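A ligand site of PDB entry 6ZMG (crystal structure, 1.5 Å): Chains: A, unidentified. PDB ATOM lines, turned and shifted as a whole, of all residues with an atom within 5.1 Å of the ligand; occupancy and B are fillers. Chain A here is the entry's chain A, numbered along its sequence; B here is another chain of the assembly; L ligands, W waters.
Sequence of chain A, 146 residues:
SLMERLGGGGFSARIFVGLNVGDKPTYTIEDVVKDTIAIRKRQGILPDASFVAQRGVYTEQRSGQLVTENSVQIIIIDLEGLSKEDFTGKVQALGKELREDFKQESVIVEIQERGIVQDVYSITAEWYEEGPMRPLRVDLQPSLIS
Residues that only touch the ligand: Phe 16 (3.4 Å), Gly 18 (3.6 Å), Gly 56 (3.3 Å), Tyr 58 (3.2 Å), Ile 108 (3.5 Å), Asp 48 of chain B (3.5 Å), Ala 49 of chain B (3.5 Å), Ile 75 of chain B (3.2 Å), Ile 76 of chain B (3.9 Å) and Leu 79 of chain B (3.3 Å).
Within 4 Å of the ligand: Phe 16, Gly 18, Asn 20, Gln 54, Gly 56, Tyr 58, Glu 69, Ser 71, Gln 104, Glu 105, Ser 106, Ile 108, Asp 48 of chain B, Ala 49 of chain B, Ser 50 of chain B, Ile 75 of chain B, Ile 76 of chain B, Ile 77 of chain B and Leu 79 of chain B.
A nitrogen (N1) of the ligand lies within hydrogen-bond range of the side-chain amide oxygen (OE1) of Gln 104.
The side-chain hydroxyl of Ser 71 is in hydrogen-bond range of an oxygen (O5) of the ligand (2.8 Å).
An oxygen (O2) of the ligand is in hydrogen-bond range of the backbone NH (N) of Glu 105.
A nitrogen (N5) of the ligand sits at hydrogen-bond distance from the backbone NH of Ile 77 of chain B.
An oxygen (O5) of the ligand lies within hydrogen-bond range of the side-chain hydroxyl (OG) of Ser 50 of chain B (2.7 Å).
N1 of the ligand lies within salt-bridge range of OE1 of Glu 69 (2.8 Å).
An oxygen (O1) of the ligand lies within hydrogen-bond range of the backbone NH of Ser 106.
O5 of the ligand lies within hydrogen-bond range of NE2 of Gln 54, 3.2 Å away.
O of Ile 77 of chain B is in hydrogen-bond range of N4 of the ligand (2.8 Å).
N6 of the ligand sits at hydrogen-bond distance from N of Ser 50 of chain B, at 3.5 Å.
O of Asn 20 sits at hydrogen-bond distance from N1 of the ligand.
Water W2 lies within hydrogen-bond range of O2 of the ligand (2.7 Å), O of Lys 103 (2.9 Å) and N of Gly 22 (3.1 Å).
Water W5 lies within hydrogen-bond range of OD2 of Asp 48 of chain B (2.7 Å) and N3 of the ligand (2.7 Å).
Water W4 lies within hydrogen-bond range of O of Gly 22 and N1 of the ligand.
Water W3 lies within hydrogen-bond range of O of Ser 106 (2.6 Å), OE1 of Gln 104 (2.7 Å) and N of Gly 18 (2.8 Å).
N of Val 57 sits at hydrogen-bond distance from O of Ala 49 of chain B (2.9 Å).
The backbone carbonyl oxygen (O) of Ser 71 lies within hydrogen-bond range of the backbone NH (N) of Gln 54, at 2.9 Å.
NE2 of Gln 104 is in hydrogen-bond range of O of Asn 20, 2.9 Å away.
The backbone NH (N) of Asn 20 sits at hydrogen-bond distance from the side-chain carboxylate (OE1) of Glu 69 (3.1 Å).
OG of Ser 50 of chain B sits at hydrogen-bond distance from NE2 of Gln 54 (3.3 Å).
The side-chain hydroxyl of Ser 106 lies within hydrogen-bond range of the side-chain hydroxyl of Tyr 58 (2.8 Å).
The backbone carbonyl oxygen (O) of Ile 108 lies within hydrogen-bond range of the backbone NH (N) of Phe 16 (2.8 Å).
N of Ile 75 of chain B lies within hydrogen-bond range of O of Ser 50 of chain B, 2.8 Å away.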
ATOM      1  N   PHE A  16       3.088 -13.688 -10.071  1.00  0.00           N
ATOM      2  CA  PHE A  16       4.367 -13.003  -9.915  1.00  0.00           C
ATOM      3  C   PHE A  16       4.770 -13.021  -8.454  1.00  0.00           C
ATOM      4  O   PHE A  16       4.029 -12.499  -7.605  1.00  0.00           O
ATOM      5  CB  PHE A  16       4.278 -11.584 -10.407  1.00  0.00           C
ATOM      6  CG  PHE A  16       3.943 -11.465 -11.863  1.00  0.00           C
ATOM      7  CD1 PHE A  16       2.636 -11.474 -12.324  1.00  0.00           C
ATOM      8  CD2 PHE A  16       4.949 -11.387 -12.793  1.00  0.00           C
ATOM      9  CE1 PHE A  16       2.355 -11.358 -13.698  1.00  0.00           C
ATOM     10  CE2 PHE A  16       4.684 -11.249 -14.149  1.00  0.00           C
ATOM     11  CZ  PHE A  16       3.397 -11.236 -14.605  1.00  0.00           C
ATOM     12  N   VAL A  17       5.945 -13.582  -8.170  1.00  0.00           N
ATOM     13  CA  VAL A  17       6.471 -13.734  -6.818  1.00  0.00           C
ATOM     14  C   VAL A  17       7.860 -13.130  -6.765  1.00  0.00           C
ATOM     15  O   VAL A  17       8.753 -13.572  -7.509  1.00  0.00           O
ATOM     16  CB  VAL A  17       6.592 -15.217  -6.387  1.00  0.00           C
ATOM     17  CG1 VAL A  17       7.021 -15.301  -4.921  1.00  0.00           C
ATOM     18  CG2 VAL A  17       5.321 -15.972  -6.624  1.00  0.00           C
ATOM     19  N   GLY A  18       8.046 -12.129  -5.916  1.00  0.00           N
ATOM     20  CA  GLY A  18       9.355 -11.527  -5.739  1.00  0.00           C
ATOM     21  C   GLY A  18      10.240 -12.337  -4.806  1.00  0.00           C
ATOM     22  O   GLY A  18       9.776 -13.172  -4.043  1.00  0.00           O
ATOM     23  N   LEU A  19      11.551 -12.084  -4.921  1.00  0.00           N
ATOM     24  CA  LEU A  19      12.553 -12.822  -4.174  1.00  0.00           C
ATOM     25  C   LEU A  19      13.313 -11.961  -3.177  1.00  0.00           C
ATOM     26  O   LEU A  19      14.153 -12.482  -2.433  1.00  0.00           O
ATOM     27  CB  LEU A  19      13.523 -13.537  -5.112  1.00  0.00           C
ATOM     28  CG  LEU A  19      12.841 -14.465  -6.118  1.00  0.00           C
ATOM     29  CD1 LEU A  19      13.809 -14.995  -7.136  1.00  0.00           C
ATOM     30  CD2 LEU A  19      12.158 -15.635  -5.448  1.00  0.00           C
ATOM     31  N   ASN A  20      13.027 -10.660  -3.135  1.00  0.00           N
ATOM     32  CA  ASN A  20      13.466  -9.807  -2.047  1.00  0.00           C
ATOM     33  C   ASN A  20      12.491  -9.935  -0.883  1.00  0.00           C
ATOM     34  O   ASN A  20      11.273 -10.052  -1.089  1.00  0.00           O
ATOM     35  CB  ASN A  20      13.435  -8.329  -2.437  1.00  0.00           C
ATOM     36  CG  ASN A  20      14.724  -7.826  -3.034  1.00  0.00           C
ATOM     37  OD1 ASN A  20      15.556  -8.571  -3.531  1.00  0.00           O
ATOM     38  ND2 ASN A  20      14.887  -6.516  -2.980  1.00  0.00           N
ATOM     39  N   GLY A  22      11.612  -7.284   1.744  1.00  0.00           N
ATOM     40  CA  GLY A  22      11.938  -5.879   1.831  1.00  0.00           C
ATOM     41  C   GLY A  22      12.961  -5.492   0.782  1.00  0.00           C
ATOM     42  O   GLY A  22      12.812  -5.803  -0.399  1.00  0.00           O
ATOM     43  N   GLN A  54      12.983 -13.269 -13.679  1.00  0.00           N
ATOM     44  CA  GLN A  54      12.802 -11.905 -14.112  1.00  0.00           C
ATOM     45  C   GLN A  54      13.581 -10.982 -13.188  1.00  0.00           C
ATOM     46  O   GLN A  54      13.943 -11.348 -12.069  1.00  0.00           O
ATOM     47  CB  GLN A  54      11.347 -11.438 -13.940  1.00  0.00           C
ATOM     48  CG  GLN A  54      10.308 -12.432 -14.344  1.00  0.00           C
ATOM     49  CD  GLN A  54       8.924 -11.819 -14.331  1.00  0.00           C
ATOM     50  OE1 GLN A  54       8.227 -11.835 -15.344  1.00  0.00           O
ATOM     51  NE2 GLN A  54       8.493 -11.336 -13.175  1.00  0.00           N
ATOM     52  N   ARG A  55      13.756  -9.762 -13.663  1.00  0.00           N
ATOM     53  CA  ARG A  55      14.002  -8.618 -12.798  1.00  0.00           C
ATOM     54  C   ARG A  55      12.680  -7.879 -12.643  1.00  0.00           C
ATOM     55  O   ARG A  55      11.954  -7.674 -13.606  1.00  0.00           O
ATOM     56  CB  ARG A  55      15.064  -7.693 -13.394  1.00  0.00           C
ATOM     57  CG  ARG A  55      16.443  -8.336 -13.488  1.00  0.00           C
ATOM     58  CD  ARG A  55      17.080  -8.573 -12.142  1.00  0.00           C
ATOM     59  NE  ARG A  55      17.608  -7.340 -11.600  1.00  0.00           N
ATOM     60  CZ  ARG A  55      17.935  -7.163 -10.329  1.00  0.00           C
ATOM     61  NH1 ARG A  55      17.763  -8.138  -9.434  1.00  0.00           N
ATOM     62  NH2 ARG A  55      18.425  -5.994  -9.956  1.00  0.00           N
ATOM     63  N   GLY A  56      12.373  -7.501 -11.407  1.00  0.00           N
ATOM     64  CA  GLY A  56      11.130  -6.831 -11.106  1.00  0.00           C
ATOM     65  C   GLY A  56      11.414  -5.498 -10.450  1.00  0.00           C
ATOM     66  O   GLY A  56      12.365  -5.358  -9.689  1.00  0.00           O
ATOM     67  N   VAL A  57      10.559  -4.522 -10.750  1.00  0.00           N
ATOM     68  CA  VAL A  57      10.566  -3.218 -10.099  1.00  0.00           C
ATOM     69  C   VAL A  57       9.229  -3.062  -9.407  1.00  0.00           C
ATOM     70  O   VAL A  57       8.179  -3.285 -10.022  1.00  0.00           O
ATOM     71  CB  VAL A  57      10.780  -2.117 -11.131  1.00  0.00           C
ATOM     72  CG1 VAL A  57      10.660  -0.755 -10.454  1.00  0.00           C
ATOM     73  CG2 VAL A  57      12.126  -2.294 -11.782  1.00  0.00           C
ATOM     74  N   TYR A  58       9.257  -2.663  -8.120  1.00  0.00           N
ATOM     75  CA  TYR A  58       8.078  -2.611  -7.256  1.00  0.00           C
ATOM     76  C   TYR A  58       8.154  -1.437  -6.295  1.00  0.00           C
ATOM     77  O   TYR A  58       9.200  -1.192  -5.675  1.00  0.00           O
ATOM     78  CB  TYR A  58       7.985  -3.898  -6.420  1.00  0.00           C
ATOM     79  CG  TYR A  58       6.887  -3.971  -5.362  1.00  0.00           C
ATOM     80  CD1 TYR A  58       5.544  -4.101  -5.729  1.00  0.00           C
ATOM     81  CD2 TYR A  58       7.204  -3.961  -4.001  1.00  0.00           C
ATOM     82  CE1 TYR A  58       4.543  -4.183  -4.775  1.00  0.00           C
ATOM     83  CE2 TYR A  58       6.202  -4.051  -3.032  1.00  0.00           C
ATOM     84  CZ  TYR A  58       4.880  -4.176  -3.423  1.00  0.00           C
ATOM     85  OH  TYR A  58       3.911  -4.284  -2.450  1.00  0.00           O
ATOM     86  N   GLU A  69      14.310  -6.162  -7.740  1.00  0.00           N
ATOM     87  CA  GLU A  69      14.574  -7.476  -7.190  1.00  0.00           C
ATOM     88  C   GLU A  69      14.630  -8.489  -8.322  1.00  0.00           C
ATOM     89  O   GLU A  69      14.232  -8.221  -9.452  1.00  0.00           O
ATOM     90  CB  GLU A  69      13.473  -7.914  -6.211  1.00  0.00           C
ATOM     91  CG  GLU A  69      12.091  -7.952  -6.861  1.00  0.00           C
ATOM     92  CD  GLU A  69      10.969  -8.371  -5.905  1.00  0.00           C
ATOM     93  OE1 GLU A  69      11.237  -8.679  -4.728  1.00  0.00           O
ATOM     94  OE2 GLU A  69       9.788  -8.350  -6.345  1.00  0.00           O
ATOM     95  N   ASN A  70      15.123  -9.675  -8.002  1.00  0.00           N
ATOM     96  CA  ASN A  70      14.804 -10.823  -8.829  1.00  0.00           C
ATOM     97  C   ASN A  70      13.381 -11.265  -8.504  1.00  0.00           C
ATOM     98  O   ASN A  70      12.952 -11.196  -7.349  1.00  0.00           O
ATOM     99  CB  ASN A  70      15.754 -11.968  -8.526  1.00  0.00           C
ATOM    100  CG  ASN A  70      17.185 -11.670  -8.912  1.00  0.00           C
ATOM    101  OD1 ASN A  70      17.459 -10.915  -9.858  1.00  0.00           O
ATOM    102  ND2 ASN A  70      18.115 -12.281  -8.209  1.00  0.00           N
ATOM    103  N   SER A  71      12.675 -11.775  -9.501  1.00  0.00           N
ATOM    104  CA  SER A  71      11.330 -12.301  -9.273  1.00  0.00           C
ATOM    105  C   SER A  71      11.083 -13.472 -10.210  1.00  0.00           C
ATOM    106  O   SER A  71      11.917 -13.828 -11.058  1.00  0.00           O
ATOM    107  CB  SER A  71      10.288 -11.183  -9.387  1.00  0.00           C
ATOM    108  OG  SER A  71      10.246 -10.708 -10.701  1.00  0.00           O
ATOM    109  N   LYS A 103       7.428 -14.515   2.568  1.00  0.00           N
ATOM    110  CA  LYS A 103       7.449 -13.314   3.401  1.00  0.00           C
ATOM    111  C   LYS A 103       7.236 -12.056   2.574  1.00  0.00           C
ATOM    112  O   LYS A 103       7.884 -11.027   2.774  1.00  0.00           O
ATOM    113  CB  LYS A 103       8.727 -13.243   4.232  1.00  0.00           C
ATOM    114  CG  LYS A 103       8.876 -14.402   5.144  1.00  0.00           C
ATOM    115  CD  LYS A 103      10.117 -14.271   5.969  1.00  0.00           C
ATOM    116  CE  LYS A 103      10.229 -15.310   7.002  1.00  0.00           C
ATOM    117  NZ  LYS A 103      11.379 -14.969   7.852  1.00  0.00           N
ATOM    118  N   GLN A 104       6.328 -12.160   1.608  1.00  0.00           N
ATOM    119  CA  GLN A 104       6.102 -11.093   0.643  1.00  0.00           C
ATOM    120  C   GLN A 104       4.981 -10.171   1.074  1.00  0.00           C
ATOM    121  O   GLN A 104       3.999 -10.594   1.688  1.00  0.00           O
ATOM    122  CB  GLN A 104       5.740 -11.688  -0.728  1.00  0.00           C
ATOM    123  CG  GLN A 104       6.825 -12.551  -1.335  1.00  0.00           C
ATOM    124  CD  GLN A 104       8.032 -11.727  -1.659  1.00  0.00           C
ATOM    125  OE1 GLN A 104       7.984 -10.891  -2.564  1.00  0.00           O
ATOM    126  NE2 GLN A 104       9.112 -11.911  -0.905  1.00  0.00           N
ATOM    127  N   GLU A 105       5.100  -8.899   0.712  1.00  0.00           N
ATOM    128  CA  GLU A 105       4.014  -7.965   0.952  1.00  0.00           C
ATOM    129  C   GLU A 105       2.894  -8.144  -0.055  1.00  0.00           C
ATOM    130  O   GLU A 105       1.716  -7.996   0.286  1.00  0.00           O
ATOM    131  CB  GLU A 105       4.555  -6.544   0.902  1.00  0.00           C
ATOM    132  CG  GLU A 105       3.584  -5.461   1.225  1.00  0.00           C
ATOM    133  CD  GLU A 105       4.246  -4.108   1.060  1.00  0.00           C
ATOM    134  OE1 GLU A 105       4.345  -3.564  -0.078  1.00  0.00           O
ATOM    135  OE2 GLU A 105       4.728  -3.610   2.066  1.00  0.00           O
ATOM    136  N   SER A 106       3.241  -8.417  -1.308  1.00  0.00           N
ATOM    137  CA  SER A 106       2.255  -8.598  -2.358  1.00  0.00           C
ATOM    138  C   SER A 106       2.702  -9.748  -3.241  1.00  0.00           C
ATOM    139  O   SER A 106       3.881  -9.944  -3.490  1.00  0.00           O
ATOM    140  CB  SER A 106       2.180  -7.364  -3.290  1.00  0.00           C
ATOM    141  OG  SER A 106       1.861  -6.181  -2.593  1.00  0.00           O
ATOM    142  N   ILE A 108       1.105 -11.051  -7.130  1.00  0.00           N
ATOM    143  CA  ILE A 108       0.140 -10.714  -8.164  1.00  0.00           C
ATOM    144  C   ILE A 108      -0.312 -11.979  -8.874  1.00  0.00           C
ATOM    145  O   ILE A 108       0.522 -12.798  -9.291  1.00  0.00           O
ATOM    146  CB  ILE A 108       0.727  -9.701  -9.162  1.00  0.00           C
ATOM    147  CG1 ILE A 108       1.065  -8.408  -8.443  1.00  0.00           C
ATOM    148  CG2 ILE A 108      -0.234  -9.487 -10.312  1.00  0.00           C
ATOM    149  CD1 ILE A 108       1.899  -7.498  -9.303  1.00  0.00           C
ATOM    150  N   ASP B  48       6.527   0.393 -11.705  1.00  0.00           N
ATOM    151  CA  ASP B  48       6.499  -1.041 -11.460  1.00  0.00           C
ATOM    152  C   ASP B  48       6.286  -1.840 -12.744  1.00  0.00           C
ATOM    153  O   ASP B  48       5.409  -1.529 -13.559  1.00  0.00           O
ATOM    154  CB  ASP B  48       5.360  -1.341 -10.487  1.00  0.00           C
ATOM    155  CG  ASP B  48       5.459  -0.585  -9.152  1.00  0.00           C
ATOM    156  OD1 ASP B  48       6.056   0.511  -9.112  1.00  0.00           O
ATOM    157  OD2 ASP B  48       4.939  -1.116  -8.145  1.00  0.00           O
ATOM    158  N   ALA B  49       7.083  -2.891 -12.899  1.00  0.00           N
ATOM    159  CA  ALA B  49       7.120  -3.663 -14.127  1.00  0.00           C
ATOM    160  C   ALA B  49       7.948  -4.913 -13.897  1.00  0.00           C
ATOM    161  O   ALA B  49       8.613  -5.066 -12.866  1.00  0.00           O
ATOM    162  CB  ALA B  49       7.735  -2.856 -15.265  1.00  0.00           C
ATOM    163  N   SER B  50       7.882  -5.804 -14.866  1.00  0.00           N
ATOM    164  CA  SER B  50       8.710  -6.998 -14.913  1.00  0.00           C
ATOM    165  C   SER B  50       9.549  -6.979 -16.191  1.00  0.00           C
ATOM    166  O   SER B  50       9.098  -6.506 -17.240  1.00  0.00           O
ATOM    167  CB  SER B  50       7.861  -8.272 -14.918  1.00  0.00           C
ATOM    168  OG  SER B  50       7.124  -8.412 -13.699  1.00  0.00           O
ATOM    169  N   ILE B  75       7.180  -6.258 -19.224  1.00  0.00           N
ATOM    170  CA  ILE B  75       5.768  -6.545 -18.995  1.00  0.00           C
ATOM    171  C   ILE B  75       5.269  -5.509 -18.001  1.00  0.00           C
ATOM    172  O   ILE B  75       5.795  -5.405 -16.880  1.00  0.00           O
ATOM    173  CB  ILE B  75       5.551  -7.971 -18.445  1.00  0.00           C
ATOM    174  CG1 ILE B  75       6.143  -9.002 -19.405  1.00  0.00           C
ATOM    175  CG2 ILE B  75       4.057  -8.220 -18.169  1.00  0.00           C
ATOM    176  CD1 ILE B  75       6.184 -10.410 -18.810  1.00  0.00           C
ATOM    177  N   ILE B  76       4.235  -4.771 -18.396  1.00  0.00           N
ATOM    178  CA  ILE B  76       3.670  -3.702 -17.585  1.00  0.00           C
ATOM    179  C   ILE B  76       2.187  -3.984 -17.385  1.00  0.00           C
ATOM    180  O   ILE B  76       1.430  -3.997 -18.357  1.00  0.00           O
ATOM    181  CB  ILE B  76       3.849  -2.326 -18.239  1.00  0.00           C
ATOM    182  CG1 ILE B  76       5.327  -1.977 -18.372  1.00  0.00           C
ATOM    183  CG2 ILE B  76       3.104  -1.241 -17.430  1.00  0.00           C
ATOM    184  CD1 ILE B  76       5.603  -0.805 -19.309  1.00  0.00           C
ATOM    185  N   ILE B  77       1.778  -4.201 -16.139  1.00  0.00           N
ATOM    186  CA  ILE B  77       0.361  -4.275 -15.786  1.00  0.00           C
ATOM    187  C   ILE B  77      -0.008  -2.940 -15.165  1.00  0.00           C
ATOM    188  O   ILE B  77       0.644  -2.476 -14.217  1.00  0.00           O
ATOM    189  CB  ILE B  77       0.086  -5.426 -14.798  1.00  0.00           C
ATOM    190  CG1 ILE B  77       0.525  -6.759 -15.406  1.00  0.00           C
ATOM    191  CG2 ILE B  77      -1.396  -5.467 -14.415  1.00  0.00           C
ATOM    192  CD1 ILE B  77       0.523  -7.888 -14.445  1.00  0.00           C
ATOM    193  N   ASP B  78      -1.047  -2.287 -15.689  1.00  0.00           N
ATOM    194  CA  ASP B  78      -1.454  -1.005 -15.134  1.00  0.00           C
ATOM    195  C   ASP B  78      -2.124  -1.225 -13.794  1.00  0.00           C
ATOM    196  O   ASP B  78      -3.209  -1.809 -13.730  1.00  0.00           O
ATOM    197  CB  ASP B  78      -2.412  -0.299 -16.081  1.00  0.00           C
ATOM    198  CG  ASP B  78      -2.917   1.027 -15.521  1.00  0.00           C
ATOM    199  OD1 ASP B  78      -2.198   1.623 -14.688  1.00  0.00           O
ATOM    200  OD2 ASP B  78      -4.039   1.457 -15.906  1.00  0.00           O
ATOM    201  N   LEU B  79      -1.519  -0.754 -12.705  1.00  0.00           N
ATOM    202  CA  LEU B  79      -2.117  -0.819 -11.384  1.00  0.00           C
ATOM    203  C   LEU B  79      -2.754   0.488 -10.942  1.00  0.00           C
ATOM    204  O   LEU B  79      -3.240   0.570  -9.813  1.00  0.00           O
ATOM    205  CB  LEU B  79      -1.082  -1.188 -10.335  1.00  0.00           C
ATOM    206  CG  LEU B  79      -0.265  -2.424 -10.670  1.00  0.00           C
ATOM    207  CD1 LEU B  79       0.817  -2.594  -9.635  1.00  0.00           C
ATOM    208  CD2 LEU B  79      -1.164  -3.641 -10.782  1.00  0.00           C
HETATM  209  N1  LIG L   1       9.223  -8.495  -2.847  1.00  0.00           N
HETATM  210  C1  LIG L   1       7.982  -7.749  -3.059  1.00  0.00           C
HETATM  211  C2  LIG L   1       7.221  -8.301  -4.298  1.00  0.00           C
HETATM  212  C3  LIG L   1       6.840  -7.162  -5.217  1.00  0.00           C
HETATM  213  S1  LIG L   1       5.759  -7.612  -6.594  1.00  0.00           S
HETATM  214  C4  LIG L   1       7.016  -7.778  -1.870  1.00  0.00           C
HETATM  215  O1  LIG L   1       5.885  -7.361  -1.969  1.00  0.00           O
HETATM  216  O2  LIG L   1       7.516  -8.229  -0.771  1.00  0.00           O
HETATM  217  C5  LIG L   1       6.521  -9.110  -7.266  1.00  0.00           C
HETATM  218  C6  LIG L   1       6.863  -8.981  -8.740  1.00  0.00           C
HETATM  219  O3  LIG L   1       5.689  -8.596  -9.499  1.00  0.00           O
HETATM  220  C7  LIG L   1       7.869  -7.898  -9.089  1.00  0.00           C
HETATM  221  O4  LIG L   1       9.209  -8.280  -8.858  1.00  0.00           O
HETATM  222  C8  LIG L   1       7.606  -7.722 -10.595  1.00  0.00           C
HETATM  223  O5  LIG L   1       8.324  -8.730 -11.291  1.00  0.00           O
HETATM  224  C9  LIG L   1       6.100  -7.951 -10.692  1.00  0.00           C
HETATM  225  N2  LIG L   1       5.335  -6.717 -10.814  1.00  0.00           N
HETATM  226  C10 LIG L   1       4.916  -5.896  -9.789  1.00  0.00           C
HETATM  227  N3  LIG L   1       4.166  -4.894 -10.201  1.00  0.00           N
HETATM  228  C11 LIG L   1       4.095  -5.072 -11.575  1.00  0.00           C
HETATM  229  C12 LIG L   1       3.390  -4.396 -12.586  1.00  0.00           C
HETATM  230  N4  LIG L   1       2.605  -3.325 -12.364  1.00  0.00           N
HETATM  231  N5  LIG L   1       3.497  -4.862 -13.852  1.00  0.00           N
HETATM  232  C13 LIG L   1       4.270  -5.927 -14.071  1.00  0.00           C
HETATM  233  N6  LIG L   1       4.962  -6.662 -13.207  1.00  0.00           N
HETATM  234  C14 LIG L   1       4.829  -6.188 -11.957  1.00  0.00           C
HETATM  235  O   HOH W   1       8.253  -5.027   0.199  1.00  0.00           O
HETATM  236  O   HOH W   2       8.859  -8.613   1.535  1.00  0.00           O
HETATM  237  O   HOH W   3       5.895 -11.415  -4.258  1.00  0.00           O
HETATM  238  O   HOH W   4      10.160  -6.523  -0.996  1.00  0.00           O
HETATM  239  O   HOH W   5       3.526  -3.379  -8.026  1.00  0.00           O
